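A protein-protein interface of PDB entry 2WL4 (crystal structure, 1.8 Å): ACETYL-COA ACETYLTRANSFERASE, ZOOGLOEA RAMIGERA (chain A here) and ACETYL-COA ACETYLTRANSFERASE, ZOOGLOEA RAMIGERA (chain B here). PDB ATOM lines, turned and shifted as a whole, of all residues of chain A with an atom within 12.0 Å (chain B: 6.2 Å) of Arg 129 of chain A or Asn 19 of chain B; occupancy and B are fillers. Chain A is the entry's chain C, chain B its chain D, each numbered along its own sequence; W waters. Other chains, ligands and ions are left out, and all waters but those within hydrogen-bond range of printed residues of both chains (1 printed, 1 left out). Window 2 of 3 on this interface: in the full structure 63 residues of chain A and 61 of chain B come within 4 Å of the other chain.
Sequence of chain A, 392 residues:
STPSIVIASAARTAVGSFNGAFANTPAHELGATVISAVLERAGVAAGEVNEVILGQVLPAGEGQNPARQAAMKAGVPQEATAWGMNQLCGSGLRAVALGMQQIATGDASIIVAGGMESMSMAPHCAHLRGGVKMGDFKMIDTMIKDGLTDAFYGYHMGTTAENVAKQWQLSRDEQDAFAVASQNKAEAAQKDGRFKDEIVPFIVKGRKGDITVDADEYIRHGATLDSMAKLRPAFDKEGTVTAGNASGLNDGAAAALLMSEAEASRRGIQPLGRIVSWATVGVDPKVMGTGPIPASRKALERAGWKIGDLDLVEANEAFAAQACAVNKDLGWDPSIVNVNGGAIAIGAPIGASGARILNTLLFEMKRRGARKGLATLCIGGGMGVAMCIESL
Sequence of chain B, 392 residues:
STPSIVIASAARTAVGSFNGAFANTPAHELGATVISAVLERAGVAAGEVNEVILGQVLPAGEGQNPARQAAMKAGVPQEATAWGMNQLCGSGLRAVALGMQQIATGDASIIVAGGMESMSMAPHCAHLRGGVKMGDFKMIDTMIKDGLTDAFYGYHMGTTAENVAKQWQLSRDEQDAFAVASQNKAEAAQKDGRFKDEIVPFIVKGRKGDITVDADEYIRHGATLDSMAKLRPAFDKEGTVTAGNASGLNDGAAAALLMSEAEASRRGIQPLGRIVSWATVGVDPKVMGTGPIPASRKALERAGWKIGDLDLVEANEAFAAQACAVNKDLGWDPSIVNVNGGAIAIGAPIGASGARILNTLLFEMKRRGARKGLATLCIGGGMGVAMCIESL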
ATOM      1  N   ALA A  60     -31.490  17.369  16.254  1.00  0.00           N
ATOM      2  CA  ALA A  60     -30.051  17.297  16.052  1.00  0.00           C
ATOM      3  C   ALA A  60     -29.649  17.084  14.589  1.00  0.00           C
ATOM      4  O   ALA A  60     -30.164  16.192  13.914  1.00  0.00           O
ATOM      5  CB  ALA A  60     -29.450  16.224  16.953  1.00  0.00           C
ATOM      6  N   GLY A  61     -28.734  17.926  14.110  1.00  0.00           N
ATOM      7  CA  GLY A  61     -28.190  17.810  12.768  1.00  0.00           C
ATOM      8  C   GLY A  61     -29.052  18.373  11.647  1.00  0.00           C
ATOM      9  O   GLY A  61     -28.645  18.373  10.482  1.00  0.00           O
ATOM     10  N   HIS A 124     -27.396   9.239  14.778  1.00  0.00           N
ATOM     11  CA  HIS A 124     -26.652   8.702  15.901  1.00  0.00           C
ATOM     12  C   HIS A 124     -25.528   9.676  16.200  1.00  0.00           C
ATOM     13  O   HIS A 124     -25.011  10.328  15.291  1.00  0.00           O
ATOM     14  CB  HIS A 124     -26.068   7.337  15.552  1.00  0.00           C
ATOM     15  CG  HIS A 124     -27.094   6.256  15.422  1.00  0.00           C
ATOM     16  ND1 HIS A 124     -28.049   6.253  14.426  1.00  0.00           N
ATOM     17  CD2 HIS A 124     -27.311   5.135  16.150  1.00  0.00           C
ATOM     18  CE1 HIS A 124     -28.808   5.181  14.552  1.00  0.00           C
ATOM     19  NE2 HIS A 124     -28.381   4.484  15.592  1.00  0.00           N
ATOM     20  N   CYS A 125     -25.136   9.760  17.468  1.00  0.00           N
ATOM     21  CA  CYS A 125     -24.110  10.712  17.877  1.00  0.00           C
ATOM     22  C   CYS A 125     -23.070  10.129  18.839  1.00  0.00           C
ATOM     23  O   CYS A 125     -23.290   9.071  19.426  1.00  0.00           O
ATOM     24  CB  CYS A 125     -24.779  11.907  18.545  1.00  0.00           C
ATOM     25  SG  CYS A 125     -25.760  11.470  19.998  1.00  0.00           S
ATOM     26  N   ALA A 126     -21.952  10.839  19.007  1.00  0.00           N
ATOM     27  CA  ALA A 126     -20.975  10.501  20.029  1.00  0.00           C
ATOM     28  C   ALA A 126     -20.153  11.737  20.382  1.00  0.00           C
ATOM     29  O   ALA A 126     -19.707  12.459  19.493  1.00  0.00           O
ATOM     30  CB  ALA A 126     -20.036   9.345  19.557  1.00  0.00           C
ATOM     31  N   HIS A 127     -19.946  11.983  21.672  1.00  0.00           N
ATOM     32  CA  HIS A 127     -19.120  13.110  22.078  1.00  0.00           C
ATOM     33  C   HIS A 127     -17.657  12.814  21.785  1.00  0.00           C
ATOM     34  O   HIS A 127     -17.060  11.905  22.375  1.00  0.00           O
ATOM     35  CB  HIS A 127     -19.300  13.434  23.554  1.00  0.00           C
ATOM     36  CG  HIS A 127     -18.461  14.585  24.012  1.00  0.00           C
ATOM     37  ND1 HIS A 127     -17.762  14.574  25.201  1.00  0.00           N
ATOM     38  CD2 HIS A 127     -18.188  15.775  23.425  1.00  0.00           C
ATOM     39  CE1 HIS A 127     -17.111  15.715  25.336  1.00  0.00           C
ATOM     40  NE2 HIS A 127     -17.350  16.461  24.271  1.00  0.00           N
ATOM     41  N   LEU A 128     -17.066  13.590  20.890  1.00  0.00           N
ATOM     42  CA  LEU A 128     -15.775  13.199  20.318  1.00  0.00           C
ATOM     43  C   LEU A 128     -14.674  14.225  20.444  1.00  0.00           C
ATOM     44  O   LEU A 128     -13.596  14.057  19.867  1.00  0.00           O
ATOM     45  CB  LEU A 128     -15.962  12.870  18.842  1.00  0.00           C
ATOM     46  CG  LEU A 128     -16.849  11.674  18.541  1.00  0.00           C
ATOM     47  CD1 LEU A 128     -17.113  11.614  17.047  1.00  0.00           C
ATOM     48  CD2 LEU A 128     -16.157  10.416  19.036  1.00  0.00           C
ATOM     49  N   ARG A 129     -14.936  15.283  21.199  1.00  0.00           N
ATOM     50  CA  ARG A 129     -13.943  16.329  21.415  1.00  0.00           C
ATOM     51  C   ARG A 129     -12.687  15.849  22.152  1.00  0.00           C
ATOM     52  O   ARG A 129     -11.627  16.469  22.052  1.00  0.00           O
ATOM     53  CB  ARG A 129     -14.584  17.527  22.122  1.00  0.00           C
ATOM     54  CG  ARG A 129     -15.091  18.568  21.140  1.00  0.00           C
ATOM     55  CD  ARG A 129     -16.075  19.537  21.762  1.00  0.00           C
ATOM     56  NE  ARG A 129     -17.430  19.308  21.266  1.00  0.00           N
ATOM     57  CZ  ARG A 129     -17.809  19.522  20.011  1.00  0.00           C
ATOM     58  NH1 ARG A 129     -16.936  19.975  19.114  1.00  0.00           N
ATOM     59  NH2 ARG A 129     -19.065  19.299  19.653  1.00  0.00           N
ATOM     60  N   GLY A 130     -12.788  14.734  22.870  1.00  0.00           N
ATOM     61  CA  GLY A 130     -11.652  14.225  23.623  1.00  0.00           C
ATOM     62  C   GLY A 130     -10.586  13.595  22.747  1.00  0.00           C
ATOM     63  O   GLY A 130      -9.389  13.786  22.980  1.00  0.00           O
ATOM     64  N   GLY A 131     -11.018  12.855  21.729  1.00  0.00           N
ATOM     65  CA  GLY A 131     -10.093  12.154  20.856  1.00  0.00           C
ATOM     66  C   GLY A 131      -9.717  10.814  21.456  1.00  0.00           C
ATOM     67  O   GLY A 131      -8.630  10.656  22.007  1.00  0.00           O
ATOM     68  N   VAL A 132     -10.624   9.851  21.343  1.00  0.00           N
ATOM     69  CA  VAL A 132     -10.469   8.543  21.975  1.00  0.00           C
ATOM     70  C   VAL A 132      -9.086   7.929  21.754  1.00  0.00           C
ATOM     71  O   VAL A 132      -8.720   7.583  20.628  1.00  0.00           O
ATOM     72  CB  VAL A 132     -11.563   7.571  21.487  1.00  0.00           C
ATOM     73  CG1 VAL A 132     -11.656   6.352  22.403  1.00  0.00           C
ATOM     74  CG2 VAL A 132     -12.896   8.289  21.418  1.00  0.00           C
ATOM     75  N   LYS A 133      -8.332   7.785  22.841  1.00  0.00           N
ATOM     76  CA  LYS A 133      -6.951   7.309  22.798  1.00  0.00           C
ATOM     77  C   LYS A 133      -6.833   5.833  22.411  1.00  0.00           C
ATOM     78  O   LYS A 133      -5.928   5.448  21.665  1.00  0.00           O
ATOM     79  CB  LYS A 133      -6.277   7.542  24.144  1.00  0.00           C
ATOM     80  CG  LYS A 133      -5.034   6.714  24.332  1.00  0.00           C
ATOM     81  CD  LYS A 133      -4.815   6.362  25.793  1.00  0.00           C
ATOM     82  CE  LYS A 133      -3.995   5.097  25.904  1.00  0.00           C
ATOM     83  NZ  LYS A 133      -2.555   5.356  25.611  1.00  0.00           N
ATOM     84  N   MET A 134      -7.721   5.010  22.961  1.00  0.00           N
ATOM     85  CA  MET A 134      -7.909   3.624  22.506  1.00  0.00           C
ATOM     86  C   MET A 134      -9.182   3.010  23.079  1.00  0.00           C
ATOM     87  O   MET A 134      -9.690   3.445  24.119  1.00  0.00           O
ATOM     88  CB  MET A 134      -6.709   2.735  22.832  1.00  0.00           C
ATOM     89  CG  MET A 134      -6.636   2.244  24.273  1.00  0.00           C
ATOM     90  SD  MET A 134      -5.226   1.119  24.526  1.00  0.00           S
ATOM     91  CE  MET A 134      -5.383   0.783  26.279  1.00  0.00           C
ATOM     92  N   PHE A 137     -15.856   3.175  21.132  1.00  0.00           N
ATOM     93  CA  PHE A 137     -16.795   4.086  21.779  1.00  0.00           C
ATOM     94  C   PHE A 137     -18.155   3.951  21.110  1.00  0.00           C
ATOM     95  O   PHE A 137     -18.256   3.538  19.954  1.00  0.00           O
ATOM     96  CB  PHE A 137     -16.286   5.533  21.798  1.00  0.00           C
ATOM     97  CG  PHE A 137     -16.084   6.137  20.439  1.00  0.00           C
ATOM     98  CD1 PHE A 137     -14.875   5.999  19.775  1.00  0.00           C
ATOM     99  CD2 PHE A 137     -17.101   6.859  19.829  1.00  0.00           C
ATOM    100  CE1 PHE A 137     -14.686   6.561  18.518  1.00  0.00           C
ATOM    101  CE2 PHE A 137     -16.922   7.423  18.580  1.00  0.00           C
ATOM    102  CZ  PHE A 137     -15.716   7.276  17.923  1.00  0.00           C
ATOM    103  N   LYS A 138     -19.212   4.254  21.850  1.00  0.00           N
ATOM    104  CA  LYS A 138     -20.556   4.016  21.336  1.00  0.00           C
ATOM    105  C   LYS A 138     -21.052   5.123  20.413  1.00  0.00           C
ATOM    106  O   LYS A 138     -20.775   6.305  20.625  1.00  0.00           O
ATOM    107  CB  LYS A 138     -21.553   3.773  22.475  1.00  0.00           C
ATOM    108  CG  LYS A 138     -21.413   2.407  23.131  1.00  0.00           C
ATOM    109  CD  LYS A 138     -22.610   2.077  24.011  1.00  0.00           C
ATOM    110  CE  LYS A 138     -22.394   0.772  24.767  1.00  0.00           C
ATOM    111  NZ  LYS A 138     -23.457   0.517  25.782  1.00  0.00           N
ATOM    112  N   MET A 139     -21.759   4.712  19.366  1.00  0.00           N
ATOM    113  CA  MET A 139     -22.551   5.628  18.561  1.00  0.00           C
ATOM    114  C   MET A 139     -23.995   5.506  19.021  1.00  0.00           C
ATOM    115  O   MET A 139     -24.651   4.486  18.781  1.00  0.00           O
ATOM    116  CB  MET A 139     -22.408   5.307  17.069  1.00  0.00           C
ATOM    117  CG  MET A 139     -21.081   5.796  16.496  1.00  0.00           C
ATOM    118  SD  MET A 139     -21.051   7.591  16.462  1.00  0.00           S
ATOM    119  CE  MET A 139     -19.379   7.898  15.903  1.00  0.00           C
ATOM    120  N   SER B  17     -14.938  27.939  30.002  1.00  0.00           N
ATOM    121  CA  SER B  17     -14.306  27.935  28.691  1.00  0.00           C
ATOM    122  C   SER B  17     -14.599  26.627  27.965  1.00  0.00           C
ATOM    123  O   SER B  17     -14.997  25.643  28.583  1.00  0.00           O
ATOM    124  CB  SER B  17     -12.792  28.144  28.827  1.00  0.00           C
ATOM    125  OG  SER B  17     -12.494  29.297  29.600  1.00  0.00           O
ATOM    126  N   PHE B  18     -14.403  26.628  26.650  1.00  0.00           N
ATOM    127  CA  PHE B  18     -14.651  25.462  25.815  1.00  0.00           C
ATOM    128  C   PHE B  18     -13.683  24.332  26.178  1.00  0.00           C
ATOM    129  O   PHE B  18     -12.470  24.492  26.079  1.00  0.00           O
ATOM    130  CB  PHE B  18     -14.499  25.856  24.337  1.00  0.00           C
ATOM    131  CG  PHE B  18     -15.063  24.852  23.353  1.00  0.00           C
ATOM    132  CD1 PHE B  18     -16.244  24.173  23.614  1.00  0.00           C
ATOM    133  CD2 PHE B  18     -14.430  24.629  22.138  1.00  0.00           C
ATOM    134  CE1 PHE B  18     -16.766  23.262  22.692  1.00  0.00           C
ATOM    135  CE2 PHE B  18     -14.954  23.719  21.212  1.00  0.00           C
ATOM    136  CZ  PHE B  18     -16.124  23.040  21.493  1.00  0.00           C
ATOM    137  N   ASN B  19     -14.236  23.200  26.607  1.00  0.00           N
ATOM    138  CA  ASN B  19     -13.453  22.022  26.976  1.00  0.00           C
ATOM    139  C   ASN B  19     -12.677  22.182  28.280  1.00  0.00           C
ATOM    140  O   ASN B  19     -11.665  21.511  28.488  1.00  0.00           O
ATOM    141  CB  ASN B  19     -12.489  21.632  25.850  1.00  0.00           C
ATOM    142  CG  ASN B  19     -13.208  21.156  24.603  1.00  0.00           C
ATOM    143  OD1 ASN B  19     -12.892  20.096  24.060  1.00  0.00           O
ATOM    144  ND2 ASN B  19     -14.183  21.937  24.144  1.00  0.00           N
ATOM    145  N   GLY B  20     -13.172  23.049  29.162  1.00  0.00           N
ATOM    146  CA  GLY B  20     -12.445  23.428  30.362  1.00  0.00           C
ATOM    147  C   GLY B  20     -13.129  23.084  31.670  1.00  0.00           C
ATOM    148  O   GLY B  20     -13.313  21.908  31.992  1.00  0.00           O
ATOM    149  N   ALA B  21     -13.504  24.114  32.424  1.00  0.00           N
ATOM    150  CA  ALA B  21     -14.049  23.937  33.767  1.00  0.00           C
ATOM    151  C   ALA B  21     -15.157  22.894  33.813  1.00  0.00           C
ATOM    152  O   ALA B  21     -15.196  22.069  34.723  1.00  0.00           O
ATOM    153  CB  ALA B  21     -14.542  25.265  34.328  1.00  0.00           C
ATOM    154  N   PHE B  22     -16.057  22.939  32.833  1.00  0.00           N
ATOM    155  CA  PHE B  22     -17.128  21.954  32.744  1.00  0.00           C
ATOM    156  C   PHE B  22     -17.002  21.121  31.462  1.00  0.00           C
ATOM    157  O   PHE B  22     -17.996  20.836  30.789  1.00  0.00           O
ATOM    158  CB  PHE B  22     -18.497  22.630  32.811  1.00  0.00           C
ATOM    159  CG  PHE B  22     -18.616  23.684  33.896  1.00  0.00           C
ATOM    160  CD1 PHE B  22     -18.038  23.493  35.146  1.00  0.00           C
ATOM    161  CD2 PHE B  22     -19.324  24.855  33.665  1.00  0.00           C
ATOM    162  CE1 PHE B  22     -18.149  24.460  36.140  1.00  0.00           C
ATOM    163  CE2 PHE B  22     -19.447  25.827  34.657  1.00  0.00           C
ATOM    164  CZ  PHE B  22     -18.857  25.632  35.893  1.00  0.00           C
ATOM    165  N   ALA B  23     -15.772  20.733  31.134  1.00  0.00           N
ATOM    166  CA  ALA B  23     -15.493  19.987  29.907  1.00  0.00           C
ATOM    167  C   ALA B  23     -16.368  18.752  29.789  1.00  0.00           C
ATOM    168  O   ALA B  23     -16.943  18.471  28.729  1.00  0.00           O
ATOM    169  CB  ALA B  23     -14.021  19.587  29.852  1.00  0.00           C
ATOM    170  N   ASN B  24     -16.462  18.013  30.888  1.00  0.00           N
ATOM    171  CA  ASN B  24     -17.193  16.759  30.895  1.00  0.00           C
ATOM    172  C   ASN B  24     -18.469  16.809  31.740  1.00  0.00           C
ATOM    173  O   ASN B  24     -18.968  15.771  32.162  1.00  0.00           O
ATOM    174  CB  ASN B  24     -16.280  15.628  31.384  1.00  0.00           C
ATOM    175  CG  ASN B  24     -14.817  15.852  31.012  1.00  0.00           C
ATOM    176  OD1 ASN B  24     -14.494  16.199  29.874  1.00  0.00           O
ATOM    177  ND2 ASN B  24     -13.926  15.645  31.976  1.00  0.00           N
ATOM    178  N   MET B 119     -21.895  23.618  25.539  1.00  0.00           N
ATOM    179  CA  MET B 119     -21.379  23.500  24.188  1.00  0.00           C
ATOM    180  C   MET B 119     -20.247  22.466  24.128  1.00  0.00           C
ATOM    181  O   MET B 119     -20.071  21.780  23.122  1.00  0.00           O
ATOM    182  CB  MET B 119     -20.947  24.872  23.672  1.00  0.00           C
ATOM    183  CG  MET B 119     -22.083  25.883  23.743  1.00  0.00           C
ATOM    184  SD  MET B 119     -21.602  27.556  23.303  1.00  0.00           S
ATOM    185  CE  MET B 119     -21.411  27.354  21.516  1.00  0.00           C
ATOM    186  N   SER B 120     -19.508  22.335  25.223  1.00  0.00           N
ATOM    187  CA  SER B 120     -18.415  21.366  25.308  1.00  0.00           C
ATOM    188  C   SER B 120     -18.884  19.936  25.065  1.00  0.00           C
ATOM    189  O   SER B 120     -18.197  19.142  24.410  1.00  0.00           O
ATOM    190  CB  SER B 120     -17.754  21.444  26.685  1.00  0.00           C
ATOM    191  OG  SER B 120     -16.992  22.621  26.816  1.00  0.00           O
ATOM    192  N   MET B 121     -20.069  19.623  25.582  1.00  0.00           N
ATOM    193  CA  MET B 121     -20.597  18.257  25.567  1.00  0.00           C
ATOM    194  C   MET B 121     -21.440  17.932  24.339  1.00  0.00           C
ATOM    195  O   MET B 121     -21.910  16.812  24.187  1.00  0.00           O
ATOM    196  CB  MET B 121     -21.396  17.982  26.844  1.00  0.00           C
ATOM    197  CG  MET B 121     -20.512  17.811  28.069  1.00  0.00           C
ATOM    198  SD  MET B 121     -19.610  16.255  28.034  1.00  0.00           S
ATOM    199  CE  MET B 121     -20.935  15.095  28.381  1.00  0.00           C
ATOM    200  N   ALA B 122     -21.639  18.918  23.472  1.00  0.00           N
ATOM    201  CA  ALA B 122     -22.374  18.703  22.233  1.00  0.00           C
ATOM    202  C   ALA B 122     -21.577  17.732  21.369  1.00  0.00           C
ATOM    203  O   ALA B 122     -20.405  17.956  21.117  1.00  0.00           O
ATOM    204  CB  ALA B 122     -22.571  20.011  21.515  1.00  0.00           C
ATOM    205  N   PRO B 123     -22.222  16.650  20.913  1.00  0.00           N
ATOM    206  CA  PRO B 123     -21.553  15.536  20.241  1.00  0.00           C
ATOM    207  C   PRO B 123     -21.421  15.753  18.733  1.00  0.00           C
ATOM    208  O   PRO B 123     -21.898  16.765  18.221  1.00  0.00           O
ATOM    209  CB  PRO B 123     -22.499  14.356  20.516  1.00  0.00           C
ATOM    210  CG  PRO B 123     -23.779  14.987  21.231  1.00  0.00           C
ATOM    211  CD  PRO B 123     -23.678  16.441  21.001  1.00  0.00           C
ATOM    212  N   HIS B 124     -20.773  14.811  18.048  1.00  0.00           N
ATOM    213  CA  HIS B 124     -20.812  14.719  16.585  1.00  0.00           C
ATOM    214  C   HIS B 124     -21.834  13.674  16.174  1.00  0.00           C
ATOM    215  O   HIS B 124     -22.112  12.743  16.934  1.00  0.00           O
ATOM    216  CB  HIS B 124     -19.450  14.322  16.034  1.00  0.00           C
ATOM    217  CG  HIS B 124     -18.451  15.440  16.013  1.00  0.00           C
ATOM    218  ND1 HIS B 124     -17.964  16.032  17.161  1.00  0.00           N
ATOM    219  CD2 HIS B 124     -17.838  16.065  14.981  1.00  0.00           C
ATOM    220  CE1 HIS B 124     -17.092  16.970  16.834  1.00  0.00           C
ATOM    221  NE2 HIS B 124     -16.992  17.006  15.517  1.00  0.00           N
ATOM    222  N   ASP B 141     -21.246  18.122  14.031  1.00  0.00           N
ATOM    223  CA  ASP B 141     -20.730  18.856  15.204  1.00  0.00           C
ATOM    224  C   ASP B 141     -21.832  19.372  16.147  1.00  0.00           C
ATOM    225  O   ASP B 141     -21.561  19.744  17.292  1.00  0.00           O
ATOM    226  CB  ASP B 141     -19.824  20.024  14.773  1.00  0.00           C
ATOM    227  CG  ASP B 141     -19.332  20.852  15.947  1.00  0.00           C
ATOM    228  OD1 ASP B 141     -20.137  21.619  16.509  1.00  0.00           O
ATOM    229  OD2 ASP B 141     -18.134  20.756  16.299  1.00  0.00           O
ATOM    230  N   THR B 142     -23.067  19.385  15.661  1.00  0.00           N
ATOM    231  CA  THR B 142     -24.232  19.924  16.385  1.00  0.00           C
ATOM    232  C   THR B 142     -24.061  21.330  16.969  1.00  0.00           C
ATOM    233  O   THR B 142     -24.973  22.149  16.892  1.00  0.00           O
ATOM    234  CB  THR B 142     -24.787  18.948  17.464  1.00  0.00           C
ATOM    235  OG1 THR B 142     -23.994  19.000  18.658  1.00  0.00           O
ATOM    236  CG2 THR B 142     -24.819  17.531  16.928  1.00  0.00           C
ATOM    237  N   MET B 143     -22.905  21.608  17.558  1.00  0.00           N
ATOM    238  CA  MET B 143     -22.618  22.941  18.072  1.00  0.00           C
ATOM    239  C   MET B 143     -22.498  23.915  16.901  1.00  0.00           C
ATOM    240  O   MET B 143     -23.131  24.975  16.894  1.00  0.00           O
ATOM    241  CB  MET B 143     -21.330  22.935  18.901  1.00  0.00           C
ATOM    242  CG  MET B 143     -21.025  24.249  19.610  1.00  0.00           C
ATOM    243  SD  MET B 143     -19.275  24.409  20.025  1.00  0.00           S
ATOM    244  CE  MET B 143     -18.557  24.212  18.385  1.00  0.00           C
ATOM    245  N   GLU B 217     -13.893  31.802  33.733  1.00  0.00           N
ATOM    246  CA  GLU B 217     -12.542  31.485  33.290  1.00  0.00           C
ATOM    247  C   GLU B 217     -12.292  31.847  31.833  1.00  0.00           C
ATOM    248  O   GLU B 217     -11.306  31.411  31.234  1.00  0.00           O
ATOM    249  CB  GLU B 217     -12.260  30.005  33.503  1.00  0.00           C
ATOM    250  CG  GLU B 217     -13.128  29.099  32.660  1.00  0.00           C
ATOM    251  CD  GLU B 217     -12.721  27.651  32.782  1.00  0.00           C
ATOM    252  OE1 GLU B 217     -11.805  27.377  33.581  1.00  0.00           O
ATOM    253  OE2 GLU B 217     -13.310  26.795  32.085  1.00  0.00           O
ATOM    254  N   LEU B 249     -16.830  30.103  22.773  1.00  0.00           N
ATOM    255  CA  LEU B 249     -17.675  28.929  22.898  1.00  0.00           C
ATOM    256  C   LEU B 249     -17.608  28.516  24.364  1.00  0.00           C
ATOM    257  O   LEU B 249     -16.510  28.367  24.918  1.00  0.00           O
ATOM    258  CB  LEU B 249     -17.161  27.817  21.999  1.00  0.00           C
ATOM    259  CG  LEU B 249     -16.901  28.231  20.548  1.00  0.00           C
ATOM    260  CD1 LEU B 249     -15.874  27.323  19.877  1.00  0.00           C
ATOM    261  CD2 LEU B 249     -18.195  28.263  19.754  1.00  0.00           C
ATOM    262  N   ASP B 251     -19.673  27.007  28.334  1.00  0.00           N
ATOM    263  CA  ASP B 251     -20.629  26.203  29.089  1.00  0.00           C
ATOM    264  C   ASP B 251     -21.146  26.921  30.334  1.00  0.00           C
ATOM    265  O   ASP B 251     -20.392  27.597  31.040  1.00  0.00           O
ATOM    266  CB  ASP B 251     -19.993  24.875  29.515  1.00  0.00           C
ATOM    267  CG  ASP B 251     -19.259  24.186  28.384  1.00  0.00           C
ATOM    268  OD1 ASP B 251     -19.673  24.337  27.213  1.00  0.00           O
ATOM    269  OD2 ASP B 251     -18.265  23.484  28.675  1.00  0.00           O
HETATM  270  O   HOH W   1     -18.493  16.050  20.164  1.00  0.00           O
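N of Ala 126 of chain A is in hydrogen-bond range of O of His 124 of chain B, 2.8 Å away.
A ring nitrogen (NE2) of His 127 of chain A sits at hydrogen-bond distance from the backbone carbonyl oxygen of Ser 120 of chain B (2.8 Å).
ND1 of His 127 of chain A sits close to SD of Met 121 of chain B, 3.8 Å away.
The backbone carbonyl oxygen (O) of Ser 120 of chain B is in hydrogen-bond range of the guanidinium group (NE) of Arg 129 of chain A (3.2 Å).
The guanidinium group (NE) of Arg 129 of chain A sits close to the backbone carbonyl oxygen (O) of Ala 122 of chain B (3.3 Å).
OD2 of Asp 141 of chain B is in salt-bridge range of NH1 of Arg 129 of chain A.
N of Phe 18 of chain B lies within hydrogen-bond range of O of Leu 249 of chain B, 3.2 Å away.
N of Asn 19 of chain B is in hydrogen-bond range of OG of Ser 120 of chain B (2.8 Å).
OD2 of Asp 251 of chain B is in hydrogen-bond range of OG of Ser 120 of chain B (2.4 Å).
O of Pro 123 of chain B sits at hydrogen-bond distance from OG1 of Thr 142 of chain B, 3.1 Å away.
N of Met 143 of chain B lies close to OD1 of Asp 141 of chain B (3.0 Å).
Cys 125 of chain A touches Pro 123 of chain B (CB to CB, 3.9 Å).
Cys 125 of chain A touches His 124 of chain B (CA to O, 3.0 Å).
Ala 126 of chain A touches Pro 123 of chain B (C to CB, 3.5 Å).
Ala 122 of chain B touches His 127 of chain A (O to CD2, 3.9 Å).
Pro 123 of chain B touches His 127 of chain A (CB to N, 3.7 Å).
CD1 of Leu 128 of chain A touches CB of His 124 of chain B, at 3.7 Å.
CD of Arg 129 of chain A touches CZ of Phe 18 of chain B (3.5 Å).
Arg 129 of chain A touches Asn 19 of chain B.
Arg 129 of chain A touches His 124 of chain B.
Printed residues of chain B within 4 Å of Ala 126 of chain A: Pro 123 and His 124.
Of the printed residues of chain B, His 127 of chain A touches Ser 120, Met 121, Ala 122 and Pro 123.
Of the printed residues of chain B, Leu 128 of chain A touches His 124.
Arg 129 of chain A touches just these residues of chain B: Phe 18, Asn 19, Ser 120, Ala 122, His 124 and Asp 141.
Val 132 of chain A touches none of the printed residues of chain B.
Ser 17 of chain B touches none of the printed residues of chain A.
Phe 18 of chain B touches just one residue of chain A: Arg 129.
Asn 19 of chain B touches just one residue of chain A: Arg 129 (3.6 Å).
No residue of chain A comes within 4 Å of Gly 20 of chain B.
No residue of chain A comes within 4 Å of Ala 21 of chain B.
No residue of chain A comes within 4 Å of Ala 23 of chain B.
Printed residues of chain A within 4 Å of Ser 120 of chain B: His 127 and Arg 129.
Of the printed residues of chain A, Met 121 of chain B touches His 127.
His 124 of chain B touches just these residues of chain A: Cys 125, Ala 126, Leu 128 and Arg 129.
Asp 141 of chain B touches one residue of chain A.
No residue of chain A comes within 4 Å of Thr 142 of chain B.
No residue of chain A comes within 4 Å of Met 143 of chain B.
Glu 217 of chain B touches none of the printed residues of chain A.
The nearest printed residue of chain B that does not touch Arg 129 of chain A is Pro 123 of chain B (4.1 Å).
The nearest residue of chain A that does not touch Asn 19 of chain B is Gly 130 of chain A (5.5 Å).
The nearest printed residue of chain B that does not touch Leu 128 of chain A is Pro 123 of chain B (4.9 Å).
Hydrophobic or aromatic side chains of chain B that line the printed part of chain A: Phe 18, Met 121, Pro 123 and His 124.
Of the 16 printed residues of chain A, 5 touch a printed residue of chain B.
Hydrophobic or aromatic side chains of chain A within 4 Å of the printed part of chain B: His 127 and Leu 128.
Among the printed residues, Asp or Glu carboxylates within 4 Å of a Lys or Arg side-chain nitrogen of the other chain: Arg 129 of chain A with Asp 141 of chain B (3.2 Å).
Water W1 lies within hydrogen-bond range of the backbone carbonyl oxygen of Ala 122 of chain B (2.9 Å), the backbone NH of Leu 128 of chain A (2.9 Å), a ring nitrogen (ND1) of His 124 of chain B (3.0 Å) and the guanidinium group of Arg 129 of chain A (3.3 Å).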
